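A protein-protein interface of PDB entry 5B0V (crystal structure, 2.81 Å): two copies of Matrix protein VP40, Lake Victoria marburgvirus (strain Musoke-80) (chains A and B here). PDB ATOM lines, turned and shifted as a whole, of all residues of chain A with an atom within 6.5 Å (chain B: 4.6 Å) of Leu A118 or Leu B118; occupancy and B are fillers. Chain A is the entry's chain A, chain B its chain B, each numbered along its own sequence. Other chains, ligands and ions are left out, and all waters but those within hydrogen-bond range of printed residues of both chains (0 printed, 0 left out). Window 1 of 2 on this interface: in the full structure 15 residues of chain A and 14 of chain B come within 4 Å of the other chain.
The backbone NH (N) of Leu B183 lies within hydrogen-bond range of the backbone carbonyl oxygen (O) of Asn B56 (2.7 Å).
The backbone carbonyl oxygen of Ala A116 is in hydrogen-bond range of the side-chain hydroxyl of Thr A119.
The side-chain hydroxyl of Thr A119 is in hydrogen-bond range of the backbone carbonyl oxygen of Ala A115.
O of Ala B115 sits at hydrogen-bond distance from OG1 of Thr B119.
The backbone carbonyl oxygen (O) of Asn A56 lies within hydrogen-bond range of the backbone NH (N) of Leu A183.
Of the printed residues of chain B, Asn A56 touches Thr B54, Pro B55 and Asn B56.
Of the printed residues of chain B, Tyr A57 touches Thr B54 (3.0 Å), Leu B118 (3.7 Å) and Thr B119 (3.4 Å).
Leu A118 touches two residues of chain B.
Ser A121 touches none of the printed residues of chain B.
Of the printed residues of chain A, Asn B56 touches Thr A54 (3.0 Å), Pro A55 (3.9 Å) and Asn A56 (3.3 Å).
Printed residues of chain A within 4 Å of Tyr B57: Thr A54 (3.3 Å), Leu A118 (3.8 Å) and Thr A119 (3.6 Å).
Of the printed residues of chain A, Leu B118 touches Tyr A57 (3.7 Å) and Leu A118 (3.8 Å).
Printed residues of chain A within 4 Å of Thr B119: Tyr A57 (3.4 Å) and Val A114 (3.99 Å).
The nearest residue of chain A that does not touch Leu B118 is Thr A119 (4.1 Å).
The nearest printed residue of chain B that does not touch Tyr A57 is Pro B55 (4.7 Å).
Hydrophobic or aromatic side chains of chain A that line the printed part of chain B: Tyr A57, Val A114 and Leu A118.
Among the printed residues, 13 pairs touch across the chains.
The side-chain hydroxyl (OG1) of Thr B54 sits at hydrogen-bond distance from the backbone NH (N) of Tyr A57 (3.0 Å).
The side-chain hydroxyl (OG1) of Thr A54 lies within hydrogen-bond range of the backbone NH (N) of Tyr B57 (3.3 Å).
The side-chain amide nitrogen (ND2) of Asn A56 lies within hydrogen-bond range of the side-chain amide oxygen (OD1) of Asn B56, at 3.3 Å.
ND2 of Asn B56 lies within hydrogen-bond range of O of Thr A54 (3.0 Å).
Thr A54 touches Asn B56, and with the chains exchanged Asn A56 touches Thr B54.
Pro A55 touches Asn B56, and with the chains exchanged Asn A56 touches Pro B55.
Tyr A57 touches Thr B119, and with the chains exchanged Thr A119 touches Tyr B57.
Val A114 touches Thr B119, but with the chains exchanged Thr A119 does not touch Val B114 (4.2 Å).
Positions printed for both chains: 54, 55, 56, 57, 114, 115, 116, 117, 118, 119, 120 and 183.
Of the 13 pairs that touch across the chains among the printed residues, 12 have their exchanged pair printed and touching as well.
Among the printed residues, pairs that only touch across the chains: Pro A55 with Asn B56, Asn A56 with Thr B54, Asn A56 with Pro B55, Tyr A57 with Leu B118, Tyr A57 with Thr B119, Val A114 with Thr B119, Leu A118 with Tyr B57, Leu A118 with Leu B118 and Thr A119 with Tyr B57.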
ATOM      1  N   THR A  54      12.930 -22.927  20.190  1.00  0.00           N
ATOM      2  CA  THR A  54      13.815 -22.454  21.243  1.00  0.00           C
ATOM      3  C   THR A  54      15.203 -23.049  21.090  1.00  0.00           C
ATOM      4  O   THR A  54      15.366 -24.134  20.611  1.00  0.00           O
ATOM      5  CB  THR A  54      13.260 -22.706  22.673  1.00  0.00           C
ATOM      6  OG1 THR A  54      13.583 -24.030  23.101  1.00  0.00           O
ATOM      7  CG2 THR A  54      11.752 -22.516  22.717  1.00  0.00           C
ATOM      8  N   PRO A  55      16.217 -22.330  21.537  1.00  0.00           N
ATOM      9  CA  PRO A  55      17.532 -22.849  21.316  1.00  0.00           C
ATOM     10  C   PRO A  55      18.002 -23.763  22.415  1.00  0.00           C
ATOM     11  O   PRO A  55      17.381 -23.879  23.466  1.00  0.00           O
ATOM     12  CB  PRO A  55      18.395 -21.587  21.295  1.00  0.00           C
ATOM     13  CG  PRO A  55      17.664 -20.617  22.163  1.00  0.00           C
ATOM     14  CD  PRO A  55      16.229 -21.033  22.234  1.00  0.00           C
ATOM     15  N   ASN A  56      19.134 -24.386  22.189  1.00  0.00           N
ATOM     16  CA  ASN A  56      19.822 -24.974  23.308  1.00  0.00           C
ATOM     17  C   ASN A  56      21.217 -24.413  23.323  1.00  0.00           C
ATOM     18  O   ASN A  56      21.588 -23.607  22.482  1.00  0.00           O
ATOM     19  CB  ASN A  56      19.793 -26.500  23.273  1.00  0.00           C
ATOM     20  CG  ASN A  56      20.305 -27.038  21.985  1.00  0.00           C
ATOM     21  OD1 ASN A  56      21.438 -26.796  21.622  1.00  0.00           O
ATOM     22  ND2 ASN A  56      19.451 -27.742  21.261  1.00  0.00           N
ATOM     23  N   TYR A  57      21.988 -24.804  24.309  1.00  0.00           N
ATOM     24  CA  TYR A  57      23.110 -23.987  24.704  1.00  0.00           C
ATOM     25  C   TYR A  57      24.412 -24.679  24.418  1.00  0.00           C
ATOM     26  O   TYR A  57      24.520 -25.907  24.450  1.00  0.00           O
ATOM     27  CB  TYR A  57      23.003 -23.629  26.209  1.00  0.00           C
ATOM     28  CG  TYR A  57      24.290 -23.155  26.829  1.00  0.00           C
ATOM     29  CD1 TYR A  57      24.719 -21.837  26.674  1.00  0.00           C
ATOM     30  CD2 TYR A  57      25.097 -24.027  27.526  1.00  0.00           C
ATOM     31  CE1 TYR A  57      25.918 -21.401  27.228  1.00  0.00           C
ATOM     32  CE2 TYR A  57      26.292 -23.610  28.089  1.00  0.00           C
ATOM     33  CZ  TYR A  57      26.705 -22.296  27.943  1.00  0.00           C
ATOM     34  OH  TYR A  57      27.909 -21.908  28.494  1.00  0.00           O
ATOM     35  N   VAL A  58      25.407 -23.859  24.144  1.00  0.00           N
ATOM     36  CA  VAL A  58      26.757 -24.328  24.062  1.00  0.00           C
ATOM     37  C   VAL A  58      27.623 -23.144  24.441  1.00  0.00           C
ATOM     38  O   VAL A  58      27.321 -22.020  24.037  1.00  0.00           O
ATOM     39  CB  VAL A  58      27.047 -24.881  22.641  1.00  0.00           C
ATOM     40  CG1 VAL A  58      27.005 -23.783  21.588  1.00  0.00           C
ATOM     41  CG2 VAL A  58      28.388 -25.579  22.610  1.00  0.00           C
ATOM     42  N   THR A 113      19.570 -12.584  31.619  1.00  0.00           N
ATOM     43  CA  THR A 113      19.925 -12.479  30.209  1.00  0.00           C
ATOM     44  C   THR A 113      19.923 -13.851  29.551  1.00  0.00           C
ATOM     45  O   THR A 113      19.301 -14.051  28.513  1.00  0.00           O
ATOM     46  CB  THR A 113      21.304 -11.810  30.014  1.00  0.00           C
ATOM     47  OG1 THR A 113      21.316 -10.520  30.654  1.00  0.00           O
ATOM     48  CG2 THR A 113      21.590 -11.663  28.548  1.00  0.00           C
ATOM     49  N   VAL A 114      20.613 -14.792  30.185  1.00  0.00           N
ATOM     50  CA  VAL A 114      20.734 -16.130  29.646  1.00  0.00           C
ATOM     51  C   VAL A 114      19.399 -16.889  29.685  1.00  0.00           C
ATOM     52  O   VAL A 114      19.046 -17.602  28.741  1.00  0.00           O
ATOM     53  CB  VAL A 114      21.820 -16.927  30.385  1.00  0.00           C
ATOM     54  CG1 VAL A 114      21.851 -18.374  29.887  1.00  0.00           C
ATOM     55  CG2 VAL A 114      23.173 -16.253  30.194  1.00  0.00           C
ATOM     56  N   ALA A 115      18.655 -16.731  30.767  1.00  0.00           N
ATOM     57  CA  ALA A 115      17.364 -17.399  30.881  1.00  0.00           C
ATOM     58  C   ALA A 115      16.408 -16.860  29.834  1.00  0.00           C
ATOM     59  O   ALA A 115      15.668 -17.617  29.201  1.00  0.00           O
ATOM     60  CB  ALA A 115      16.796 -17.196  32.268  1.00  0.00           C
ATOM     61  N   ALA A 116      16.448 -15.545  29.650  1.00  0.00           N
ATOM     62  CA  ALA A 116      15.584 -14.884  28.694  1.00  0.00           C
ATOM     63  C   ALA A 116      15.881 -15.376  27.269  1.00  0.00           C
ATOM     64  O   ALA A 116      14.985 -15.536  26.444  1.00  0.00           O
ATOM     65  CB  ALA A 116      15.759 -13.389  28.795  1.00  0.00           C
ATOM     66  N   LEU A 117      17.149 -15.613  26.983  1.00  0.00           N
ATOM     67  CA  LEU A 117      17.554 -15.983  25.637  1.00  0.00           C
ATOM     68  C   LEU A 117      17.136 -17.414  25.368  1.00  0.00           C
ATOM     69  O   LEU A 117      16.494 -17.695  24.370  1.00  0.00           O
ATOM     70  CB  LEU A 117      19.069 -15.784  25.451  1.00  0.00           C
ATOM     71  CG  LEU A 117      19.524 -14.340  25.145  1.00  0.00           C
ATOM     72  CD1 LEU A 117      21.035 -14.221  25.203  1.00  0.00           C
ATOM     73  CD2 LEU A 117      19.011 -13.864  23.793  1.00  0.00           C
ATOM     74  N   LEU A 118      17.448 -18.309  26.294  1.00  0.00           N
ATOM     75  CA  LEU A 118      17.152 -19.725  26.104  1.00  0.00           C
ATOM     76  C   LEU A 118      15.670 -20.072  26.299  1.00  0.00           C
ATOM     77  O   LEU A 118      15.243 -21.139  25.883  1.00  0.00           O
ATOM     78  CB  LEU A 118      18.009 -20.561  27.043  1.00  0.00           C
ATOM     79  CG  LEU A 118      19.508 -20.496  26.787  1.00  0.00           C
ATOM     80  CD1 LEU A 118      20.272 -21.120  27.938  1.00  0.00           C
ATOM     81  CD2 LEU A 118      19.852 -21.189  25.480  1.00  0.00           C
ATOM     82  N   THR A 119      14.877 -19.197  26.917  1.00  0.00           N
ATOM     83  CA  THR A 119      13.445 -19.469  26.988  1.00  0.00           C
ATOM     84  C   THR A 119      12.678 -18.938  25.776  1.00  0.00           C
ATOM     85  O   THR A 119      11.526 -19.297  25.584  1.00  0.00           O
ATOM     86  CB  THR A 119      12.802 -18.972  28.303  1.00  0.00           C
ATOM     87  OG1 THR A 119      13.139 -17.600  28.549  1.00  0.00           O
ATOM     88  CG2 THR A 119      13.265 -19.843  29.469  1.00  0.00           C
ATOM     89  N   GLY A 120      13.320 -18.119  24.939  1.00  0.00           N
ATOM     90  CA  GLY A 120      12.633 -17.512  23.812  1.00  0.00           C
ATOM     91  C   GLY A 120      12.331 -18.479  22.673  1.00  0.00           C
ATOM     92  O   GLY A 120      13.121 -19.384  22.385  1.00  0.00           O
ATOM     93  N   SER A 121      11.177 -18.279  22.039  1.00  0.00           N
ATOM     94  CA  SER A 121      10.834 -18.930  20.790  1.00  0.00           C
ATOM     95  C   SER A 121      11.185 -17.992  19.650  1.00  0.00           C
ATOM     96  O   SER A 121      10.712 -16.845  19.622  1.00  0.00           O
ATOM     97  CB  SER A 121       9.343 -19.225  20.735  1.00  0.00           C
ATOM     98  OG  SER A 121       9.060 -20.505  21.281  1.00  0.00           O
ATOM     99  N   TYR A 122      11.969 -18.477  18.686  1.00  0.00           N
ATOM    100  CA  TYR A 122      12.397 -17.660  17.568  1.00  0.00           C
ATOM    101  C   TYR A 122      11.833 -18.031  16.187  1.00  0.00           C
ATOM    102  O   TYR A 122      11.536 -19.182  15.898  1.00  0.00           O
ATOM    103  CB  TYR A 122      13.917 -17.638  17.524  1.00  0.00           C
ATOM    104  CG  TYR A 122      14.531 -17.168  18.811  1.00  0.00           C
ATOM    105  CD1 TYR A 122      14.699 -18.040  19.872  1.00  0.00           C
ATOM    106  CD2 TYR A 122      14.925 -15.844  18.979  1.00  0.00           C
ATOM    107  CE1 TYR A 122      15.263 -17.623  21.063  1.00  0.00           C
ATOM    108  CE2 TYR A 122      15.492 -15.422  20.171  1.00  0.00           C
ATOM    109  CZ  TYR A 122      15.651 -16.319  21.216  1.00  0.00           C
ATOM    110  OH  TYR A 122      16.209 -15.922  22.406  1.00  0.00           O
ATOM    111  N   VAL A 182      20.880 -22.909  18.142  1.00  0.00           N
ATOM    112  CA  VAL A 182      21.792 -23.055  19.267  1.00  0.00           C
ATOM    113  C   VAL A 182      22.301 -21.663  19.696  1.00  0.00           C
ATOM    114  O   VAL A 182      22.737 -20.869  18.856  1.00  0.00           O
ATOM    115  CB  VAL A 182      23.003 -23.944  18.925  1.00  0.00           C
ATOM    116  CG1 VAL A 182      24.059 -23.878  20.032  1.00  0.00           C
ATOM    117  CG2 VAL A 182      22.584 -25.371  18.715  1.00  0.00           C
ATOM    118  N   LEU A 183      22.216 -21.382  21.002  1.00  0.00           N
ATOM    119  CA  LEU A 183      22.773 -20.173  21.574  1.00  0.00           C
ATOM    120  C   LEU A 183      24.163 -20.417  22.119  1.00  0.00           C
ATOM    121  O   LEU A 183      24.330 -21.123  23.127  1.00  0.00           O
ATOM    122  CB  LEU A 183      21.913 -19.701  22.710  1.00  0.00           C
ATOM    123  CG  LEU A 183      22.508 -18.535  23.504  1.00  0.00           C
ATOM    124  CD1 LEU A 183      22.468 -17.235  22.710  1.00  0.00           C
ATOM    125  CD2 LEU A 183      21.763 -18.394  24.809  1.00  0.00           C
ATOM    126  N   THR B  54      22.493 -30.597  26.069  1.00  0.00           N
ATOM    127  CA  THR B  54      21.758 -29.587  26.786  1.00  0.00           C
ATOM    128  C   THR B  54      20.313 -29.505  26.347  1.00  0.00           C
ATOM    129  O   THR B  54      19.971 -29.834  25.243  1.00  0.00           O
ATOM    130  CB  THR B  54      22.402 -28.197  26.666  1.00  0.00           C
ATOM    131  OG1 THR B  54      21.955 -27.542  25.480  1.00  0.00           O
ATOM    132  CG2 THR B  54      23.912 -28.296  26.678  1.00  0.00           C
ATOM    133  N   PRO B  55      19.444 -29.053  27.232  1.00  0.00           N
ATOM    134  CA  PRO B  55      18.049 -29.158  26.878  1.00  0.00           C
ATOM    135  C   PRO B  55      17.532 -27.936  26.180  1.00  0.00           C
ATOM    136  O   PRO B  55      18.231 -26.927  26.123  1.00  0.00           O
ATOM    137  CB  PRO B  55      17.366 -29.303  28.237  1.00  0.00           C
ATOM    138  CG  PRO B  55      18.283 -28.643  29.202  1.00  0.00           C
ATOM    139  CD  PRO B  55      19.653 -28.629  28.630  1.00  0.00           C
ATOM    140  N   ASN B  56      16.326 -28.079  25.635  1.00  0.00           N
ATOM    141  CA  ASN B  56      15.501 -27.030  25.075  1.00  0.00           C
ATOM    142  C   ASN B  56      14.410 -26.750  26.053  1.00  0.00           C
ATOM    143  O   ASN B  56      14.093 -27.594  26.845  1.00  0.00           O
ATOM    144  CB  ASN B  56      14.814 -27.530  23.814  1.00  0.00           C
ATOM    145  CG  ASN B  56      15.776 -27.737  22.697  1.00  0.00           C
ATOM    146  OD1 ASN B  56      16.629 -28.633  22.726  1.00  0.00           O
ATOM    147  ND2 ASN B  56      15.686 -26.879  21.722  1.00  0.00           N
ATOM    148  N   TYR B  57      13.769 -25.611  25.942  1.00  0.00           N
ATOM    149  CA  TYR B  57      12.812 -25.236  26.928  1.00  0.00           C
ATOM    150  C   TYR B  57      11.418 -25.334  26.356  1.00  0.00           C
ATOM    151  O   TYR B  57      11.179 -25.092  25.177  1.00  0.00           O
ATOM    152  CB  TYR B  57      13.114 -23.814  27.433  1.00  0.00           C
ATOM    153  CG  TYR B  57      11.952 -23.178  28.126  1.00  0.00           C
ATOM    154  CD1 TYR B  57      11.656 -23.486  29.451  1.00  0.00           C
ATOM    155  CD2 TYR B  57      11.117 -22.313  27.451  1.00  0.00           C
ATOM    156  CE1 TYR B  57      10.569 -22.921  30.091  1.00  0.00           C
ATOM    157  CE2 TYR B  57      10.028 -21.748  28.078  1.00  0.00           C
ATOM    158  CZ  TYR B  57       9.760 -22.044  29.399  1.00  0.00           C
ATOM    159  OH  TYR B  57       8.662 -21.479  30.009  1.00  0.00           O
ATOM    160  N   VAL B 114      16.906 -21.316  36.365  1.00  0.00           N
ATOM    161  CA  VAL B 114      16.580 -21.663  34.990  1.00  0.00           C
ATOM    162  C   VAL B 114      17.821 -21.627  34.089  1.00  0.00           C
ATOM    163  O   VAL B 114      17.987 -22.487  33.231  1.00  0.00           O
ATOM    164  CB  VAL B 114      15.488 -20.739  34.444  1.00  0.00           C
ATOM    165  CG1 VAL B 114      15.237 -21.016  32.969  1.00  0.00           C
ATOM    166  CG2 VAL B 114      14.209 -20.899  35.260  1.00  0.00           C
ATOM    167  N   ALA B 115      18.690 -20.647  34.288  1.00  0.00           N
ATOM    168  CA  ALA B 115      19.892 -20.540  33.488  1.00  0.00           C
ATOM    169  C   ALA B 115      20.787 -21.725  33.766  1.00  0.00           C
ATOM    170  O   ALA B 115      21.370 -22.300  32.846  1.00  0.00           O
ATOM    171  CB  ALA B 115      20.627 -19.241  33.799  1.00  0.00           C
ATOM    172  N   ALA B 116      20.871 -22.096  35.041  1.00  0.00           N
ATOM    173  CA  ALA B 116      21.676 -23.228  35.463  1.00  0.00           C
ATOM    174  C   ALA B 116      21.165 -24.548  34.849  1.00  0.00           C
ATOM    175  O   ALA B 116      21.937 -25.389  34.434  1.00  0.00           O
ATOM    176  CB  ALA B 116      21.688 -23.314  36.967  1.00  0.00           C
ATOM    177  N   LEU B 117      19.863 -24.687  34.748  1.00  0.00           N
ATOM    178  CA  LEU B 117      19.296 -25.899  34.248  1.00  0.00           C
ATOM    179  C   LEU B 117      19.519 -25.992  32.746  1.00  0.00           C
ATOM    180  O   LEU B 117      19.996 -27.004  32.247  1.00  0.00           O
ATOM    181  CB  LEU B 117      17.806 -25.969  34.598  1.00  0.00           C
ATOM    182  CG  LEU B 117      17.504 -26.442  36.031  1.00  0.00           C
ATOM    183  CD1 LEU B 117      16.022 -26.281  36.338  1.00  0.00           C
ATOM    184  CD2 LEU B 117      17.933 -27.890  36.252  1.00  0.00           C
ATOM    185  N   LEU B 118      19.208 -24.918  32.032  1.00  0.00           N
ATOM    186  CA  LEU B 118      19.322 -24.925  30.584  1.00  0.00           C
ATOM    187  C   LEU B 118      20.765 -24.849  30.090  1.00  0.00           C
ATOM    188  O   LEU B 118      21.017 -25.128  28.914  1.00  0.00           O
ATOM    189  CB  LEU B 118      18.485 -23.803  29.968  1.00  0.00           C
ATOM    190  CG  LEU B 118      16.982 -23.949  30.164  1.00  0.00           C
ATOM    191  CD1 LEU B 118      16.269 -22.652  29.783  1.00  0.00           C
ATOM    192  CD2 LEU B 118      16.419 -25.114  29.355  1.00  0.00           C
ATOM    193  N   THR B 119      21.713 -24.460  30.927  1.00  0.00           N
ATOM    194  CA  THR B 119      23.101 -24.473  30.471  1.00  0.00           C
ATOM    195  C   THR B 119      23.780 -25.808  30.717  1.00  0.00           C
ATOM    196  O   THR B 119      24.869 -26.046  30.209  1.00  0.00           O
ATOM    197  CB  THR B 119      23.944 -23.297  31.026  1.00  0.00           C
ATOM    198  OG1 THR B 119      23.808 -23.187  32.452  1.00  0.00           O
ATOM    199  CG2 THR B 119      23.502 -21.975  30.365  1.00  0.00           C
ATOM    200  N   GLY B 120      23.139 -26.686  31.473  1.00  0.00           N
ATOM    201  CA  GLY B 120      23.768 -27.932  31.830  1.00  0.00           C
ATOM    202  C   GLY B 120      23.821 -28.929  30.692  1.00  0.00           C
ATOM    203  O   GLY B 120      22.891 -29.027  29.883  1.00  0.00           O
ATOM    204  N   LEU B 183      13.601 -29.298  28.877  1.00  0.00           N
ATOM    205  CA  LEU B 183      13.229 -28.858  30.206  1.00  0.00           C
ATOM    206  C   LEU B 183      11.875 -28.178  30.201  1.00  0.00           C
ATOM    207  O   LEU B 183      11.735 -27.081  29.696  1.00  0.00           O
ATOM    208  CB  LEU B 183      14.256 -27.875  30.721  1.00  0.00           C
ATOM    209  CG  LEU B 183      13.886 -27.213  32.044  1.00  0.00           C
ATOM    210  CD1 LEU B 183      14.016 -28.189  33.223  1.00  0.00           C
ATOM    211  CD2 LEU B 183      14.782 -25.999  32.257  1.00  0.00           C
